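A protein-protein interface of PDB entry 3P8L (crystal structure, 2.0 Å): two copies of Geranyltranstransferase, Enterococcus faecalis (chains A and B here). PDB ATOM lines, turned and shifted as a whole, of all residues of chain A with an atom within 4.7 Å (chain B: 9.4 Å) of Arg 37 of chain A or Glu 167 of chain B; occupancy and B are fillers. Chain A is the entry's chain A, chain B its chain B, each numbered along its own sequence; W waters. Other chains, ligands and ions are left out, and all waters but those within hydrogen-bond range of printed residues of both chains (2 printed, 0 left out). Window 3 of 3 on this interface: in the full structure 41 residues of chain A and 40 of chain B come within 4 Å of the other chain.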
ATOM      1  N   ASN A  35       4.779  23.953  20.254  1.00  0.00           N
ATOM      2  CA  ASN A  35       4.712  23.786  18.807  1.00  0.00           C
ATOM      3  C   ASN A  35       3.261  23.842  18.326  1.00  0.00           C
ATOM      4  O   ASN A  35       2.420  23.062  18.786  1.00  0.00           O
ATOM      5  CB  ASN A  35       5.396  22.469  18.406  1.00  0.00           C
ATOM      6  CG  ASN A  35       5.422  22.250  16.898  1.00  0.00           C
ATOM      7  OD1 ASN A  35       4.449  21.812  16.314  1.00  0.00           O
ATOM      8  ND2 ASN A  35       6.562  22.525  16.278  1.00  0.00           N
ATOM      9  N   GLU A  36       2.973  24.785  17.424  1.00  0.00           N
ATOM     10  CA  GLU A  36       1.606  25.003  16.914  1.00  0.00           C
ATOM     11  C   GLU A  36       1.022  23.804  16.174  1.00  0.00           C
ATOM     12  O   GLU A  36      -0.145  23.499  16.339  1.00  0.00           O
ATOM     13  CB  GLU A  36       1.517  26.263  16.031  1.00  0.00           C
ATOM     14  CG  GLU A  36       1.834  27.569  16.767  1.00  0.00           C
ATOM     15  CD  GLU A  36       0.903  27.836  17.960  1.00  0.00           C
ATOM     16  OE1 GLU A  36      -0.272  27.416  17.947  1.00  0.00           O
ATOM     17  OE2 GLU A  36       1.348  28.486  18.925  1.00  0.00           O
ATOM     18  N   ARG A  37       1.833  23.119  15.376  1.00  0.00           N
ATOM     19  CA  ARG A  37       1.353  21.955  14.626  1.00  0.00           C
ATOM     20  C   ARG A  37       0.994  20.782  15.537  1.00  0.00           C
ATOM     21  O   ARG A  37      -0.047  20.139  15.336  1.00  0.00           O
ATOM     22  CB  ARG A  37       2.383  21.494  13.597  1.00  0.00           C
ATOM     23  CG  ARG A  37       2.006  20.147  12.952  1.00  0.00           C
ATOM     24  CD  ARG A  37       3.051  19.699  11.970  1.00  0.00           C
ATOM     25  NE  ARG A  37       2.641  18.519  11.218  1.00  0.00           N
ATOM     26  CZ  ARG A  37       1.959  18.587  10.068  1.00  0.00           C
ATOM     27  NH1 ARG A  37       1.615  19.766   9.575  1.00  0.00           N
ATOM     28  NH2 ARG A  37       1.617  17.492   9.407  1.00  0.00           N
ATOM     29  N   LEU A  38       1.867  20.510  16.515  1.00  0.00           N
ATOM     30  CA  LEU A  38       1.617  19.493  17.531  1.00  0.00           C
ATOM     31  C   LEU A  38       0.316  19.792  18.277  1.00  0.00           C
ATOM     32  O   LEU A  38      -0.541  18.916  18.412  1.00  0.00           O
ATOM     33  CB  LEU A  38       2.797  19.397  18.504  1.00  0.00           C
ATOM     34  CG  LEU A  38       2.611  18.312  19.569  1.00  0.00           C
ATOM     35  CD1 LEU A  38       2.733  16.899  18.951  1.00  0.00           C
ATOM     36  CD2 LEU A  38       3.564  18.517  20.767  1.00  0.00           C
ATOM     37  N   LYS A  39       0.184  21.039  18.734  1.00  0.00           N
ATOM     38  CA  LYS A  39      -1.035  21.562  19.354  1.00  0.00           C
ATOM     39  C   LYS A  39      -2.297  21.309  18.514  1.00  0.00           C
ATOM     40  O   LYS A  39      -3.281  20.756  18.997  1.00  0.00           O
ATOM     41  CB  LYS A  39      -0.865  23.054  19.623  1.00  0.00           C
ATOM     42  CG  LYS A  39      -2.071  23.736  20.259  1.00  0.00           C
ATOM     43  CD  LYS A  39      -1.954  25.267  20.197  1.00  0.00           C
ATOM     44  CE  LYS A  39      -0.769  25.768  21.035  1.00  0.00           C
ATOM     45  NZ  LYS A  39      -0.668  27.261  21.017  1.00  0.00           N
ATOM     46  N   GLU A  40      -2.248  21.663  17.235  1.00  0.00           N
ATOM     47  CA  GLU A  40      -3.409  21.463  16.349  1.00  0.00           C
ATOM     48  C   GLU A  40      -3.763  20.005  16.117  1.00  0.00           C
ATOM     49  O   GLU A  40      -4.931  19.647  15.997  1.00  0.00           O
ATOM     50  CB  GLU A  40      -3.165  22.129  14.994  1.00  0.00           C
ATOM     51  CG  GLU A  40      -3.412  23.611  15.020  1.00  0.00           C
ATOM     52  CD  GLU A  40      -2.894  24.284  13.765  1.00  0.00           C
ATOM     53  OE1 GLU A  40      -3.129  23.718  12.676  1.00  0.00           O
ATOM     54  OE2 GLU A  40      -2.241  25.348  13.865  1.00  0.00           O
ATOM     55  N   ALA A  41      -2.749  19.164  16.069  1.00  0.00           N
ATOM     56  CA  ALA A  41      -2.982  17.752  15.844  1.00  0.00           C
ATOM     57  C   ALA A  41      -3.627  17.097  17.076  1.00  0.00           C
ATOM     58  O   ALA A  41      -4.566  16.290  16.948  1.00  0.00           O
ATOM     59  CB  ALA A  41      -1.691  17.076  15.464  1.00  0.00           C
ATOM     60  N   PHE A 112      -2.475  14.350   9.444  1.00  0.00           N
ATOM     61  CA  PHE A 112      -1.229  15.062   9.732  1.00  0.00           C
ATOM     62  C   PHE A 112       0.039  14.290   9.395  1.00  0.00           C
ATOM     63  O   PHE A 112       1.146  14.818   9.535  1.00  0.00           O
ATOM     64  CB  PHE A 112      -1.190  15.485  11.212  1.00  0.00           C
ATOM     65  CG  PHE A 112      -2.259  16.475  11.595  1.00  0.00           C
ATOM     66  CD1 PHE A 112      -2.122  17.826  11.288  1.00  0.00           C
ATOM     67  CD2 PHE A 112      -3.405  16.048  12.259  1.00  0.00           C
ATOM     68  CE1 PHE A 112      -3.119  18.762  11.638  1.00  0.00           C
ATOM     69  CE2 PHE A 112      -4.412  16.949  12.606  1.00  0.00           C
ATOM     70  CZ  PHE A 112      -4.265  18.328  12.304  1.00  0.00           C
ATOM     71  N   THR A 116       3.557  13.023  13.036  1.00  0.00           N
ATOM     72  CA  THR A 116       2.783  13.980  13.834  1.00  0.00           C
ATOM     73  C   THR A 116       1.798  13.276  14.804  1.00  0.00           C
ATOM     74  O   THR A 116       1.646  13.702  15.938  1.00  0.00           O
ATOM     75  CB  THR A 116       2.054  14.963  12.944  1.00  0.00           C
ATOM     76  OG1 THR A 116       3.009  15.659  12.128  1.00  0.00           O
ATOM     77  CG2 THR A 116       1.293  16.005  13.777  1.00  0.00           C
ATOM     78  N   ASN B 155       4.659  18.319  25.915  1.00  0.00           N
ATOM     79  CA  ASN B 155       4.268  19.442  25.023  1.00  0.00           C
ATOM     80  C   ASN B 155       5.017  20.748  25.202  1.00  0.00           C
ATOM     81  O   ASN B 155       5.172  21.519  24.255  1.00  0.00           O
ATOM     82  CB  ASN B 155       2.770  19.707  25.135  1.00  0.00           C
ATOM     83  CG  ASN B 155       1.945  18.537  24.684  1.00  0.00           C
ATOM     84  OD1 ASN B 155       2.399  17.740  23.873  1.00  0.00           O
ATOM     85  ND2 ASN B 155       0.732  18.417  25.205  1.00  0.00           N
ATOM     86  N   VAL B 159       8.682  16.807  23.082  1.00  0.00           N
ATOM     87  CA  VAL B 159       7.724  16.453  22.015  1.00  0.00           C
ATOM     88  C   VAL B 159       7.522  17.621  21.031  1.00  0.00           C
ATOM     89  O   VAL B 159       7.474  17.405  19.803  1.00  0.00           O
ATOM     90  CB  VAL B 159       6.366  15.854  22.554  1.00  0.00           C
ATOM     91  CG1 VAL B 159       5.457  15.439  21.428  1.00  0.00           C
ATOM     92  CG2 VAL B 159       6.608  14.625  23.457  1.00  0.00           C
ATOM     93  N   SER B 160       7.439  18.847  21.548  1.00  0.00           N
ATOM     94  CA  SER B 160       7.355  20.044  20.672  1.00  0.00           C
ATOM     95  C   SER B 160       8.677  20.202  19.914  1.00  0.00           C
ATOM     96  O   SER B 160       8.674  20.517  18.717  1.00  0.00           O
ATOM     97  CB  SER B 160       7.088  21.310  21.491  1.00  0.00           C
ATOM     98  OG  SER B 160       5.712  21.452  21.826  1.00  0.00           O
ATOM     99  N   GLY B 161       9.794  19.968  20.613  1.00  0.00           N
ATOM    100  CA  GLY B 161      11.125  19.976  19.975  1.00  0.00           C
ATOM    101  C   GLY B 161      11.236  18.976  18.838  1.00  0.00           C
ATOM    102  O   GLY B 161      11.702  19.310  17.751  1.00  0.00           O
ATOM    103  N   GLN B 162      10.770  17.752  19.076  1.00  0.00           N
ATOM    104  CA  GLN B 162      10.773  16.716  18.041  1.00  0.00           C
ATOM    105  C   GLN B 162       9.928  17.100  16.824  1.00  0.00           C
ATOM    106  O   GLN B 162      10.352  16.890  15.681  1.00  0.00           O
ATOM    107  CB  GLN B 162      10.311  15.359  18.576  1.00  0.00           C
ATOM    108  CG  GLN B 162      11.301  14.614  19.452  1.00  0.00           C
ATOM    109  CD  GLN B 162      10.604  13.577  20.341  1.00  0.00           C
ATOM    110  OE1 GLN B 162       9.900  13.922  21.293  1.00  0.00           O
ATOM    111  NE2 GLN B 162      10.799  12.307  20.027  1.00  0.00           N
ATOM    112  N   MET B 163       8.756  17.682  17.072  1.00  0.00           N
ATOM    113  CA  MET B 163       7.904  18.164  15.991  1.00  0.00           C
ATOM    114  C   MET B 163       8.584  19.289  15.196  1.00  0.00           C
ATOM    115  O   MET B 163       8.546  19.280  13.967  1.00  0.00           O
ATOM    116  CB  MET B 163       6.535  18.624  16.518  1.00  0.00           C
ATOM    117  CG  MET B 163       5.454  18.821  15.417  1.00  0.00           C
ATOM    118  SD  MET B 163       4.696  17.390  14.619  1.00  0.00           S
ATOM    119  CE  MET B 163       5.844  17.025  13.264  1.00  0.00           C
ATOM    120  N   GLY B 164       9.206  20.234  15.901  1.00  0.00           N
ATOM    121  CA  GLY B 164       9.886  21.369  15.267  1.00  0.00           C
ATOM    122  C   GLY B 164      11.043  20.937  14.386  1.00  0.00           C
ATOM    123  O   GLY B 164      11.260  21.501  13.314  1.00  0.00           O
ATOM    124  N   ASP B 165      11.767  19.915  14.839  1.00  0.00           N
ATOM    125  CA  ASP B 165      12.904  19.359  14.113  1.00  0.00           C
ATOM    126  C   ASP B 165      12.474  18.737  12.782  1.00  0.00           C
ATOM    127  O   ASP B 165      13.121  18.941  11.750  1.00  0.00           O
ATOM    128  CB  ASP B 165      13.618  18.309  14.966  1.00  0.00           C
ATOM    129  CG  ASP B 165      15.012  17.979  14.442  1.00  0.00           C
ATOM    130  OD1 ASP B 165      15.738  18.917  14.061  1.00  0.00           O
ATOM    131  OD2 ASP B 165      15.378  16.794  14.418  1.00  0.00           O
ATOM    132  N   ILE B 166      11.371  17.995  12.830  1.00  0.00           N
ATOM    133  CA  ILE B 166      10.764  17.393  11.656  1.00  0.00           C
ATOM    134  C   ILE B 166      10.237  18.454  10.690  1.00  0.00           C
ATOM    135  O   ILE B 166      10.479  18.362   9.503  1.00  0.00           O
ATOM    136  CB  ILE B 166       9.688  16.366  12.060  1.00  0.00           C
ATOM    137  CG1 ILE B 166      10.382  15.168  12.721  1.00  0.00           C
ATOM    138  CG2 ILE B 166       8.817  15.932  10.858  1.00  0.00           C
ATOM    139  CD1 ILE B 166       9.449  14.282  13.530  1.00  0.00           C
ATOM    140  N   GLU B 167       9.567  19.482  11.205  1.00  0.00           N
ATOM    141  CA  GLU B 167       9.114  20.587  10.361  1.00  0.00           C
ATOM    142  C   GLU B 167      10.305  21.234   9.612  1.00  0.00           C
ATOM    143  O   GLU B 167      10.207  21.525   8.418  1.00  0.00           O
ATOM    144  CB  GLU B 167       8.328  21.616  11.172  1.00  0.00           C
ATOM    145  CG  GLU B 167       6.948  21.128  11.629  1.00  0.00           C
ATOM    146  CD  GLU B 167       6.154  22.201  12.363  1.00  0.00           C
ATOM    147  OE1 GLU B 167       5.130  22.645  11.824  1.00  0.00           O
ATOM    148  OE2 GLU B 167       6.550  22.618  13.471  1.00  0.00           O
ATOM    149  N   GLY B 168      11.437  21.375  10.309  1.00  0.00           N
ATOM    150  CA  GLY B 168      12.672  21.932   9.755  1.00  0.00           C
ATOM    151  C   GLY B 168      13.332  21.150   8.627  1.00  0.00           C
ATOM    152  O   GLY B 168      14.338  21.597   8.078  1.00  0.00           O
ATOM    153  N   GLU B 169      12.772  19.992   8.279  1.00  0.00           N
ATOM    154  CA  GLU B 169      13.248  19.213   7.132  1.00  0.00           C
ATOM    155  C   GLU B 169      12.787  19.763   5.777  1.00  0.00           C
ATOM    156  O   GLU B 169      13.379  19.441   4.748  1.00  0.00           O
ATOM    157  CB  GLU B 169      12.853  17.739   7.266  1.00  0.00           C
ATOM    158  CG  GLU B 169      13.616  16.993   8.350  1.00  0.00           C
ATOM    159  CD  GLU B 169      13.069  15.598   8.616  1.00  0.00           C
ATOM    160  OE1 GLU B 169      11.999  15.245   8.070  1.00  0.00           O
ATOM    161  OE2 GLU B 169      13.714  14.855   9.386  1.00  0.00           O
ATOM    162  N   LYS B 170      11.727  20.569   5.775  1.00  0.00           N
ATOM    163  CA  LYS B 170      11.277  21.238   4.550  1.00  0.00           C
ATOM    164  C   LYS B 170      11.615  22.736   4.554  1.00  0.00           C
ATOM    165  O   LYS B 170      12.306  23.220   3.656  1.00  0.00           O
ATOM    166  CB  LYS B 170       9.785  20.989   4.242  1.00  0.00           C
ATOM    167  CG  LYS B 170       8.882  20.639   5.426  1.00  0.00           C
ATOM    168  CD  LYS B 170       8.315  19.213   5.334  1.00  0.00           C
ATOM    169  CE  LYS B 170       9.319  18.154   5.788  1.00  0.00           C
ATOM    170  NZ  LYS B 170       8.673  16.888   6.240  1.00  0.00           N
ATOM    171  N   VAL B 171      11.133  23.456   5.565  1.00  0.00           N
ATOM    172  CA  VAL B 171      11.436  24.879   5.733  1.00  0.00           C
ATOM    173  C   VAL B 171      12.899  25.027   6.172  1.00  0.00           C
ATOM    174  O   VAL B 171      13.429  24.166   6.873  1.00  0.00           O
ATOM    175  CB  VAL B 171      10.482  25.552   6.778  1.00  0.00           C
ATOM    176  CG1 VAL B 171      10.557  27.086   6.714  1.00  0.00           C
ATOM    177  CG2 VAL B 171       9.037  25.093   6.581  1.00  0.00           C
ATOM    178  N   SER B 172      13.550  26.098   5.726  1.00  0.00           N
ATOM    179  CA  SER B 172      14.889  26.443   6.188  1.00  0.00           C
ATOM    180  C   SER B 172      14.752  27.188   7.508  1.00  0.00           C
ATOM    181  O   SER B 172      14.098  28.236   7.571  1.00  0.00           O
ATOM    182  CB  SER B 172      15.603  27.341   5.171  1.00  0.00           C
ATOM    183  OG  SER B 172      15.205  27.048   3.842  1.00  0.00           O
ATOM    184  N   LEU B 173      15.354  26.642   8.562  1.00  0.00           N
ATOM    185  CA  LEU B 173      15.323  27.288   9.869  1.00  0.00           C
ATOM    186  C   LEU B 173      16.407  28.348   9.968  1.00  0.00           C
ATOM    187  O   LEU B 173      17.500  28.169   9.433  1.00  0.00           O
ATOM    188  CB  LEU B 173      15.500  26.262  10.993  1.00  0.00           C
ATOM    189  CG  LEU B 173      14.356  25.295  11.318  1.00  0.00           C
ATOM    190  CD1 LEU B 173      14.773  24.390  12.464  1.00  0.00           C
ATOM    191  CD2 LEU B 173      13.056  26.031  11.662  1.00  0.00           C
ATOM    192  N   GLU B 177      15.748  29.911  15.379  1.00  0.00           N
ATOM    193  CA  GLU B 177      14.738  28.869  15.284  1.00  0.00           C
ATOM    194  C   GLU B 177      15.323  27.472  15.488  1.00  0.00           C
ATOM    195  O   GLU B 177      14.721  26.649  16.180  1.00  0.00           O
ATOM    196  CB  GLU B 177      14.003  28.965  13.942  1.00  0.00           C
ATOM    197  CG  GLU B 177      12.990  30.110  13.875  1.00  0.00           C
ATOM    198  CD  GLU B 177      12.478  30.385  12.467  1.00  0.00           C
ATOM    199  OE1 GLU B 177      13.075  29.869  11.496  1.00  0.00           O
ATOM    200  OE2 GLU B 177      11.476  31.128  12.333  1.00  0.00           O
ATOM    201  N   VAL B 181      14.533  24.931  18.537  1.00  0.00           N
ATOM    202  CA  VAL B 181      14.180  23.520  18.387  1.00  0.00           C
ATOM    203  C   VAL B 181      15.010  22.679  19.363  1.00  0.00           C
ATOM    204  O   VAL B 181      14.452  21.903  20.148  1.00  0.00           O
ATOM    205  CB  VAL B 181      14.377  23.001  16.940  1.00  0.00           C
ATOM    206  CG1 VAL B 181      14.347  21.489  16.914  1.00  0.00           C
ATOM    207  CG2 VAL B 181      13.308  23.586  16.006  1.00  0.00           C
ATOM    208  N   LYS B 185      14.007  20.005  22.019  1.00  0.00           N
ATOM    209  CA  LYS B 185      14.272  18.617  21.641  1.00  0.00           C
ATOM    210  C   LYS B 185      15.313  17.909  22.512  1.00  0.00           C
ATOM    211  O   LYS B 185      15.200  16.701  22.782  1.00  0.00           O
ATOM    212  CB  LYS B 185      14.699  18.518  20.159  1.00  0.00           C
ATOM    213  CG  LYS B 185      15.000  17.098  19.733  1.00  0.00           C
ATOM    214  CD  LYS B 185      15.328  16.958  18.256  1.00  0.00           C
ATOM    215  CE  LYS B 185      15.612  15.491  17.962  1.00  0.00           C
ATOM    216  NZ  LYS B 185      15.291  15.120  16.556  1.00  0.00           N
ATOM    217  N   SER B 251      20.193  21.635   7.277  1.00  0.00           N
ATOM    218  CA  SER B 251      20.104  22.917   7.969  1.00  0.00           C
ATOM    219  C   SER B 251      20.646  22.817   9.405  1.00  0.00           C
ATOM    220  O   SER B 251      19.882  22.761  10.372  1.00  0.00           O
ATOM    221  CB  SER B 251      18.664  23.432   7.954  1.00  0.00           C
ATOM    222  OG  SER B 251      18.591  24.745   8.475  1.00  0.00           O
HETATM  223  O   HOH W   1       4.314  24.282  14.030  1.00  0.00           O
HETATM  224  O   HOH W   2       8.742  23.737  18.035  1.00  0.00           O
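N of Asn 35 of chain A sits at hydrogen-bond distance from OG of Ser 160 of chain B.
ND2 of Asn 35 of chain A sits at hydrogen-bond distance from OE2 of Glu 167 of chain B (2.8 Å).
The side-chain hydroxyl (OG1) of Thr 116 of chain A lies close to the side-chain sulfur (SD) of Met 163 of chain B, 3.5 Å away.
OD1 of Asn 35 of chain A is in hydrogen-bond range of N of Leu 38 of chain A (2.9 Å).
The side-chain amide oxygen of Asn 35 of chain A lies within hydrogen-bond range of the backbone NH of Arg 37 of chain A (3.1 Å).
The backbone carbonyl oxygen (O) of Asn 155 of chain B lies within hydrogen-bond range of the side-chain hydroxyl (OG) of Ser 160 of chain B (2.5 Å).
The side-chain hydroxyl (OG1) of Thr 116 of chain A sits at hydrogen-bond distance from the guanidinium group (NE) of Arg 37 of chain A (3.0 Å).
The backbone carbonyl oxygen (O) of Phe 112 of chain A is in hydrogen-bond range of the side-chain hydroxyl (OG1) of Thr 116 of chain A (3.3 Å).
NH2 of Arg 37 of chain A is in hydrogen-bond range of O of Phe 112 of chain A, 2.7 Å away.
Among the printed residues, pairs that only touch across the chains: Asn 35 of chain A with Met 163 of chain B (3.3 Å), Asn 35 of chain A with Gly 164 of chain B (3.5 Å), Arg 37 of chain A with Met 163 of chain B (3.9 Å), Arg 37 of chain A with Glu 167 of chain B (3.5 Å), Leu 38 of chain A with Asn 155 of chain B (3.4 Å), Leu 38 of chain A with Val 159 of chain B (3.7 Å) and Leu 38 of chain A with Ser 160 of chain B (3.8 Å).
Printed residues of chain B within 4 Å of Asn 35 of chain A: Ser 160, Met 163, Gly 164 and Glu 167.
Arg 37 of chain A touches just these residues of chain B: Met 163 (3.9 Å) and Glu 167 (3.5 Å).
Ala 41 of chain A touches none of the printed residues of chain B.
Printed residues of chain B within 4 Å of Thr 116 of chain A: Met 163.
Printed residues of chain A within 4 Å of Asn 155 of chain B: Leu 38.
Of the printed residues of chain A, Val 159 of chain B touches Leu 38.
Of the printed residues of chain A, Gly 164 of chain B touches Asn 35.
Asp 165 of chain B touches none of the printed residues of chain A.
Glu 167 of chain B touches two residues of chain A.
The nearest residue of chain B that does not touch Arg 37 of chain A is Ile 166 of chain B (6.7 Å).
The nearest printed residue of chain A that does not touch Glu 167 of chain B is Glu 36 of chain A (5.8 Å).
Printed residues of chain A that touch a printed residue of chain B: Asn 35, Arg 37, Leu 38 and Thr 116.
Of the 20 printed residues of chain B, 6 touch a printed residue of chain A.
Hydrophobic or aromatic side chains of chain B within 4 Å of the printed part of chain A: Val 159 and Met 163.
Among the printed residues, 10 pairs touch across the chains.
No position is printed for both chains.
Of the 10 pairs that touch across the chains among the printed residues, none has its exchanged pair printed and touching as well.
Water W1 lies within hydrogen-bond range of OE2 of Glu 167 of chain B (2.8 Å), N of Arg 37 of chain A (3.1 Å) and OD1 of Asn 35 of chain A (3.4 Å).
Water W2 lies within hydrogen-bond range of ND2 of Asn 35 of chain A (3.1 Å) and O of Ser 160 of chain B (3.3 Å).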
